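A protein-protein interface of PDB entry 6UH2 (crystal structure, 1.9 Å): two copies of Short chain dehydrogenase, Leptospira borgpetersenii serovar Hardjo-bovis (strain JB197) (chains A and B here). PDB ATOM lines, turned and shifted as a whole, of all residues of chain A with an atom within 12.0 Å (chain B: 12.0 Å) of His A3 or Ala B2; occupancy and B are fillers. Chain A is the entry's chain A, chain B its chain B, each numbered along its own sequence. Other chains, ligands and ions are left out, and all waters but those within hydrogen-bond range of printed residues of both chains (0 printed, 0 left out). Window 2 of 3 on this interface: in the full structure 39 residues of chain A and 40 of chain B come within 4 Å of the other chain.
A ring nitrogen (NE2) of His B4 sits at hydrogen-bond distance from a ring nitrogen (ND1) of His A3 (3.2 Å).
N of His A4 sits at hydrogen-bond distance from O of Ala B2.
The backbone NH of His B4 sits at hydrogen-bond distance from the backbone carbonyl oxygen of His A4.
A ring nitrogen (ND1) of His A5 sits at hydrogen-bond distance from a ring nitrogen (NE2) of His B6.
A ring nitrogen (NE2) of His A6 sits at hydrogen-bond distance from a ring nitrogen (ND1) of His B3, at 3.1 Å.
The backbone NH (N) of His A6 sits at hydrogen-bond distance from the backbone carbonyl oxygen (O) of His B4 (2.8 Å).
The backbone NH (N) of His B6 sits at hydrogen-bond distance from the backbone carbonyl oxygen (O) of His A6 (2.7 Å).
ND1 of His B5 sits at hydrogen-bond distance from NE2 of His A8, 3.0 Å away.
The backbone NH (N) of His A8 lies within hydrogen-bond range of the backbone carbonyl oxygen (O) of His B6.
Among the printed residues, pairs that only touch across the chains: His A3 with Ala B2, His A4 with His B3, His A5 with His B4, His A6 with His B5 and His A7 with His B6.
His A3 touches just these residues of chain B: Ala B2 and His B4.
Ala B2 touches just these residues of chain A: His A3 (3.4 Å) and His A4 (2.9 Å).
Of chain B, only His B4 (3.3 Å) and His B6 (3.0 Å) come within 4 Å of His A5.
His B4 touches four residues of chain A.
Of the printed residues of chain A, His B6 touches His A5 (3.0 Å), His A6 (2.7 Å), His A7 (3.5 Å) and His A8 (2.7 Å).
Of the printed residues of chain B, His A8 touches His B5 and His B6.
Printed residues of chain B within 4 Å of His A6: His B3, His B4, His B5 and His B6.
The nearest residue of chain B that does not touch His A3 is His B3 (5.6 Å).
The nearest residue of chain A that does not touch Ala B2 is His A5 (5.6 Å).
The nearest printed residue of chain A that does not touch His B5 is His A4 (5.4 Å).
Of the 10 printed residues of chain B, 5 touch a printed residue of chain A.
Printed residues of chain B that touch a printed residue of chain A: Ala B2, His B3, His B4, His B5 and His B6.
Hydrophobic or aromatic side chains of chain B within 4 Å of the printed part of chain A: His B3, His B4, His B5 and His B6.
Printed residues of chain A that touch a printed residue of chain B: His A3, His A4, His A5, His A6, His A7 and His A8.
His A3 touches His B4, and with the chains exchanged His A4 touches His B3.
His B4 touches its own counterpart, His A4.
His A5 touches His B4, but with the chains exchanged His A4 does not touch His B5 (5.4 Å).
His B6 touches its own counterpart, His A6.
Of the 14 pairs that touch across the chains among the printed residues, 6 have their exchanged pair printed and touching as well.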
ATOM      1  N   HIS A   3     -19.872 -25.896  13.790  1.00  0.00           N
ATOM      2  CA  HIS A   3     -19.193 -26.829  12.894  1.00  0.00           C
ATOM      3  C   HIS A   3     -17.677 -26.775  13.064  1.00  0.00           C
ATOM      4  O   HIS A   3     -17.046 -25.745  12.819  1.00  0.00           O
ATOM      5  CB  HIS A   3     -19.556 -26.544  11.434  1.00  0.00           C
ATOM      6  CG  HIS A   3     -21.014 -26.704  11.128  1.00  0.00           C
ATOM      7  ND1 HIS A   3     -21.656 -27.922  11.186  1.00  0.00           N
ATOM      8  CD2 HIS A   3     -21.952 -25.800  10.757  1.00  0.00           C
ATOM      9  CE1 HIS A   3     -22.930 -27.760  10.870  1.00  0.00           C
ATOM     10  NE2 HIS A   3     -23.135 -26.483  10.604  1.00  0.00           N
ATOM     11  N   HIS A   4     -17.098 -27.896  13.483  1.00  0.00           N
ATOM     12  CA  HIS A   4     -15.653 -28.036  13.638  1.00  0.00           C
ATOM     13  C   HIS A   4     -15.180 -29.085  12.642  1.00  0.00           C
ATOM     14  O   HIS A   4     -15.497 -30.271  12.786  1.00  0.00           O
ATOM     15  CB  HIS A   4     -15.292 -28.422  15.072  1.00  0.00           C
ATOM     16  N   HIS A   5     -14.432 -28.653  11.630  1.00  0.00           N
ATOM     17  CA  HIS A   5     -13.942 -29.542  10.584  1.00  0.00           C
ATOM     18  C   HIS A   5     -12.523 -29.982  10.921  1.00  0.00           C
ATOM     19  O   HIS A   5     -11.629 -29.143  11.080  1.00  0.00           O
ATOM     20  CB  HIS A   5     -13.991 -28.856   9.217  1.00  0.00           C
ATOM     21  CG  HIS A   5     -15.380 -28.542   8.748  1.00  0.00           C
ATOM     22  ND1 HIS A   5     -16.194 -29.480   8.149  1.00  0.00           N
ATOM     23  CD2 HIS A   5     -16.099 -27.395   8.793  1.00  0.00           C
ATOM     24  CE1 HIS A   5     -17.354 -28.925   7.847  1.00  0.00           C
ATOM     25  NE2 HIS A   5     -17.322 -27.661   8.226  1.00  0.00           N
ATOM     26  N   HIS A   6     -12.324 -31.293  11.037  1.00  0.00           N
ATOM     27  CA  HIS A   6     -11.028 -31.887  11.345  1.00  0.00           C
ATOM     28  C   HIS A   6     -10.478 -32.541  10.087  1.00  0.00           C
ATOM     29  O   HIS A   6     -11.097 -33.463   9.546  1.00  0.00           O
ATOM     30  CB  HIS A   6     -11.142 -32.925  12.461  1.00  0.00           C
ATOM     31  CG  HIS A   6     -11.733 -32.394  13.728  1.00  0.00           C
ATOM     32  ND1 HIS A   6     -10.965 -31.865  14.742  1.00  0.00           N
ATOM     33  CD2 HIS A   6     -13.017 -32.327  14.153  1.00  0.00           C
ATOM     34  CE1 HIS A   6     -11.750 -31.486  15.734  1.00  0.00           C
ATOM     35  NE2 HIS A   6     -13.000 -31.756  15.403  1.00  0.00           N
ATOM     36  N   HIS A   7      -9.313 -32.088   9.642  1.00  0.00           N
ATOM     37  CA  HIS A   7      -8.692 -32.586   8.422  1.00  0.00           C
ATOM     38  C   HIS A   7      -7.521 -33.491   8.781  1.00  0.00           C
ATOM     39  O   HIS A   7      -6.608 -33.079   9.506  1.00  0.00           O
ATOM     40  CB  HIS A   7      -8.245 -31.428   7.531  1.00  0.00           C
ATOM     41  CG  HIS A   7      -9.376 -30.574   7.044  1.00  0.00           C
ATOM     42  ND1 HIS A   7     -10.109 -30.883   5.918  1.00  0.00           N
ATOM     43  CD2 HIS A   7      -9.909 -29.432   7.540  1.00  0.00           C
ATOM     44  CE1 HIS A   7     -11.042 -29.964   5.738  1.00  0.00           C
ATOM     45  NE2 HIS A   7     -10.941 -29.071   6.708  1.00  0.00           N
ATOM     46  N   HIS A   8      -7.557 -34.724   8.279  1.00  0.00           N
ATOM     47  CA  HIS A   8      -6.546 -35.732   8.553  1.00  0.00           C
ATOM     48  C   HIS A   8      -5.831 -36.088   7.258  1.00  0.00           C
ATOM     49  O   HIS A   8      -6.471 -36.287   6.222  1.00  0.00           O
ATOM     50  CB  HIS A   8      -7.174 -36.989   9.178  1.00  0.00           C
ATOM     51  CG  HIS A   8      -7.978 -36.719  10.413  1.00  0.00           C
ATOM     52  ND1 HIS A   8      -7.412 -36.277  11.589  1.00  0.00           N
ATOM     53  CD2 HIS A   8      -9.306 -36.834  10.657  1.00  0.00           C
ATOM     54  CE1 HIS A   8      -8.355 -36.134  12.504  1.00  0.00           C
ATOM     55  NE2 HIS A   8      -9.514 -36.463  11.963  1.00  0.00           N
ATOM     56  N   ALA B   2     -21.307 -29.544  16.077  1.00  0.00           N
ATOM     57  CA  ALA B   2     -21.094 -30.790  15.352  1.00  0.00           C
ATOM     58  C   ALA B   2     -19.663 -30.873  14.829  1.00  0.00           C
ATOM     59  O   ALA B   2     -19.081 -29.862  14.428  1.00  0.00           O
ATOM     60  CB  ALA B   2     -22.088 -30.915  14.207  1.00  0.00           C
ATOM     61  N   HIS B   3     -19.098 -32.078  14.836  1.00  0.00           N
ATOM     62  CA  HIS B   3     -17.739 -32.324  14.375  1.00  0.00           C
ATOM     63  C   HIS B   3     -17.776 -33.101  13.068  1.00  0.00           C
ATOM     64  O   HIS B   3     -18.565 -34.034  12.920  1.00  0.00           O
ATOM     65  CB  HIS B   3     -16.935 -33.102  15.424  1.00  0.00           C
ATOM     66  CG  HIS B   3     -16.721 -32.345  16.697  1.00  0.00           C
ATOM     67  ND1 HIS B   3     -15.662 -31.483  16.881  1.00  0.00           N
ATOM     68  CD2 HIS B   3     -17.438 -32.313  17.847  1.00  0.00           C
ATOM     69  CE1 HIS B   3     -15.735 -30.953  18.088  1.00  0.00           C
ATOM     70  NE2 HIS B   3     -16.802 -31.441  18.696  1.00  0.00           N
ATOM     71  N   HIS B   4     -16.923 -32.714  12.119  1.00  0.00           N
ATOM     72  CA  HIS B   4     -16.872 -33.342  10.802  1.00  0.00           C
ATOM     73  C   HIS B   4     -15.429 -33.693  10.476  1.00  0.00           C
ATOM     74  O   HIS B   4     -14.572 -32.806  10.406  1.00  0.00           O
ATOM     75  CB  HIS B   4     -17.454 -32.420   9.726  1.00  0.00           C
ATOM     76  CG  HIS B   4     -18.840 -31.944  10.025  1.00  0.00           C
ATOM     77  ND1 HIS B   4     -19.964 -32.677   9.709  1.00  0.00           N
ATOM     78  CD2 HIS B   4     -19.284 -30.812  10.619  1.00  0.00           C
ATOM     79  CE1 HIS B   4     -21.041 -32.018  10.097  1.00  0.00           C
ATOM     80  NE2 HIS B   4     -20.657 -30.883  10.655  1.00  0.00           N
ATOM     81  N   HIS B   5     -15.162 -34.977  10.262  1.00  0.00           N
ATOM     82  CA  HIS B   5     -13.812 -35.454  10.002  1.00  0.00           C
ATOM     83  C   HIS B   5     -13.618 -35.696   8.513  1.00  0.00           C
ATOM     84  O   HIS B   5     -14.480 -36.288   7.855  1.00  0.00           O
ATOM     85  CB  HIS B   5     -13.523 -36.725  10.801  1.00  0.00           C
ATOM     86  CG  HIS B   5     -13.431 -36.488  12.275  1.00  0.00           C
ATOM     87  ND1 HIS B   5     -12.284 -36.022  12.880  1.00  0.00           N
ATOM     88  CD2 HIS B   5     -14.348 -36.624  13.262  1.00  0.00           C
ATOM     89  CE1 HIS B   5     -12.494 -35.894  14.178  1.00  0.00           C
ATOM     90  NE2 HIS B   5     -13.738 -36.255  14.435  1.00  0.00           N
ATOM     91  N   HIS B   6     -12.487 -35.229   7.991  1.00  0.00           N
ATOM     92  CA  HIS B   6     -12.118 -35.371   6.590  1.00  0.00           C
ATOM     93  C   HIS B   6     -10.779 -36.086   6.498  1.00  0.00           C
ATOM     94  O   HIS B   6      -9.857 -35.797   7.267  1.00  0.00           O
ATOM     95  CB  HIS B   6     -12.024 -34.008   5.895  1.00  0.00           C
ATOM     96  CG  HIS B   6     -13.211 -33.128   6.128  1.00  0.00           C
ATOM     97  ND1 HIS B   6     -14.361 -33.214   5.374  1.00  0.00           N
ATOM     98  CD2 HIS B   6     -13.427 -32.142   7.032  1.00  0.00           C
ATOM     99  CE1 HIS B   6     -15.236 -32.323   5.806  1.00  0.00           C
ATOM    100  NE2 HIS B   6     -14.693 -31.659   6.811  1.00  0.00           N
ATOM    101  N   SER B  56     -16.247 -21.254  -2.206  1.00  0.00           N
ATOM    102  CA  SER B  56     -17.370 -21.597  -1.343  1.00  0.00           C
ATOM    103  C   SER B  56     -16.932 -22.276  -0.058  1.00  0.00           C
ATOM    104  O   SER B  56     -17.756 -22.451   0.846  1.00  0.00           O
ATOM    105  CB  SER B  56     -18.352 -22.507  -2.084  1.00  0.00           C
ATOM    106  OG  SER B  56     -19.260 -21.737  -2.852  1.00  0.00           O
ATOM    107  N   VAL B  57     -15.665 -22.653   0.037  1.00  0.00           N
ATOM    108  CA  VAL B  57     -15.098 -23.307   1.204  1.00  0.00           C
ATOM    109  C   VAL B  57     -14.040 -22.388   1.788  1.00  0.00           C
ATOM    110  O   VAL B  57     -13.294 -21.742   1.043  1.00  0.00           O
ATOM    111  CB  VAL B  57     -14.489 -24.674   0.826  1.00  0.00           C
ATOM    112  CG1 VAL B  57     -13.788 -25.307   2.024  1.00  0.00           C
ATOM    113  CG2 VAL B  57     -15.572 -25.593   0.267  1.00  0.00           C
ATOM    114  N   ASP B  58     -13.986 -22.319   3.117  1.00  0.00           N
ATOM    115  CA  ASP B  58     -12.903 -21.640   3.823  1.00  0.00           C
ATOM    116  C   ASP B  58     -11.793 -22.660   4.057  1.00  0.00           C
ATOM    117  O   ASP B  58     -11.877 -23.490   4.965  1.00  0.00           O
ATOM    118  CB  ASP B  58     -13.403 -21.048   5.138  1.00  0.00           C
ATOM    119  CG  ASP B  58     -12.323 -20.284   5.883  1.00  0.00           C
ATOM    120  OD1 ASP B  58     -11.208 -20.133   5.336  1.00  0.00           O
ATOM    121  OD2 ASP B  58     -12.585 -19.832   7.016  1.00  0.00           O
ATOM    122  N   TYR B  59     -10.736 -22.593   3.245  1.00  0.00           N
ATOM    123  CA  TYR B  59      -9.667 -23.577   3.377  1.00  0.00           C
ATOM    124  C   TYR B  59      -8.858 -23.414   4.660  1.00  0.00           C
ATOM    125  O   TYR B  59      -8.166 -24.359   5.057  1.00  0.00           O
ATOM    126  CB  TYR B  59      -8.748 -23.516   2.158  1.00  0.00           C
ATOM    127  CG  TYR B  59      -9.466 -23.867   0.881  1.00  0.00           C
ATOM    128  CD1 TYR B  59      -9.797 -25.187   0.596  1.00  0.00           C
ATOM    129  CD2 TYR B  59      -9.817 -22.887  -0.038  1.00  0.00           C
ATOM    130  CE1 TYR B  59     -10.460 -25.525  -0.565  1.00  0.00           C
ATOM    131  CE2 TYR B  59     -10.482 -23.215  -1.217  1.00  0.00           C
ATOM    132  CZ  TYR B  59     -10.801 -24.536  -1.473  1.00  0.00           C
ATOM    133  OH  TYR B  59     -11.464 -24.872  -2.636  1.00  0.00           O
ATOM    134  N   LYS B  60      -8.937 -22.253   5.317  1.00  0.00           N
ATOM    135  CA  LYS B  60      -8.250 -22.008   6.590  1.00  0.00           C
ATOM    136  C   LYS B  60      -6.766 -22.369   6.491  1.00  0.00           C
ATOM    137  O   LYS B  60      -6.207 -23.079   7.331  1.00  0.00           O
ATOM    138  CB  LYS B  60      -8.932 -22.772   7.730  1.00  0.00           C
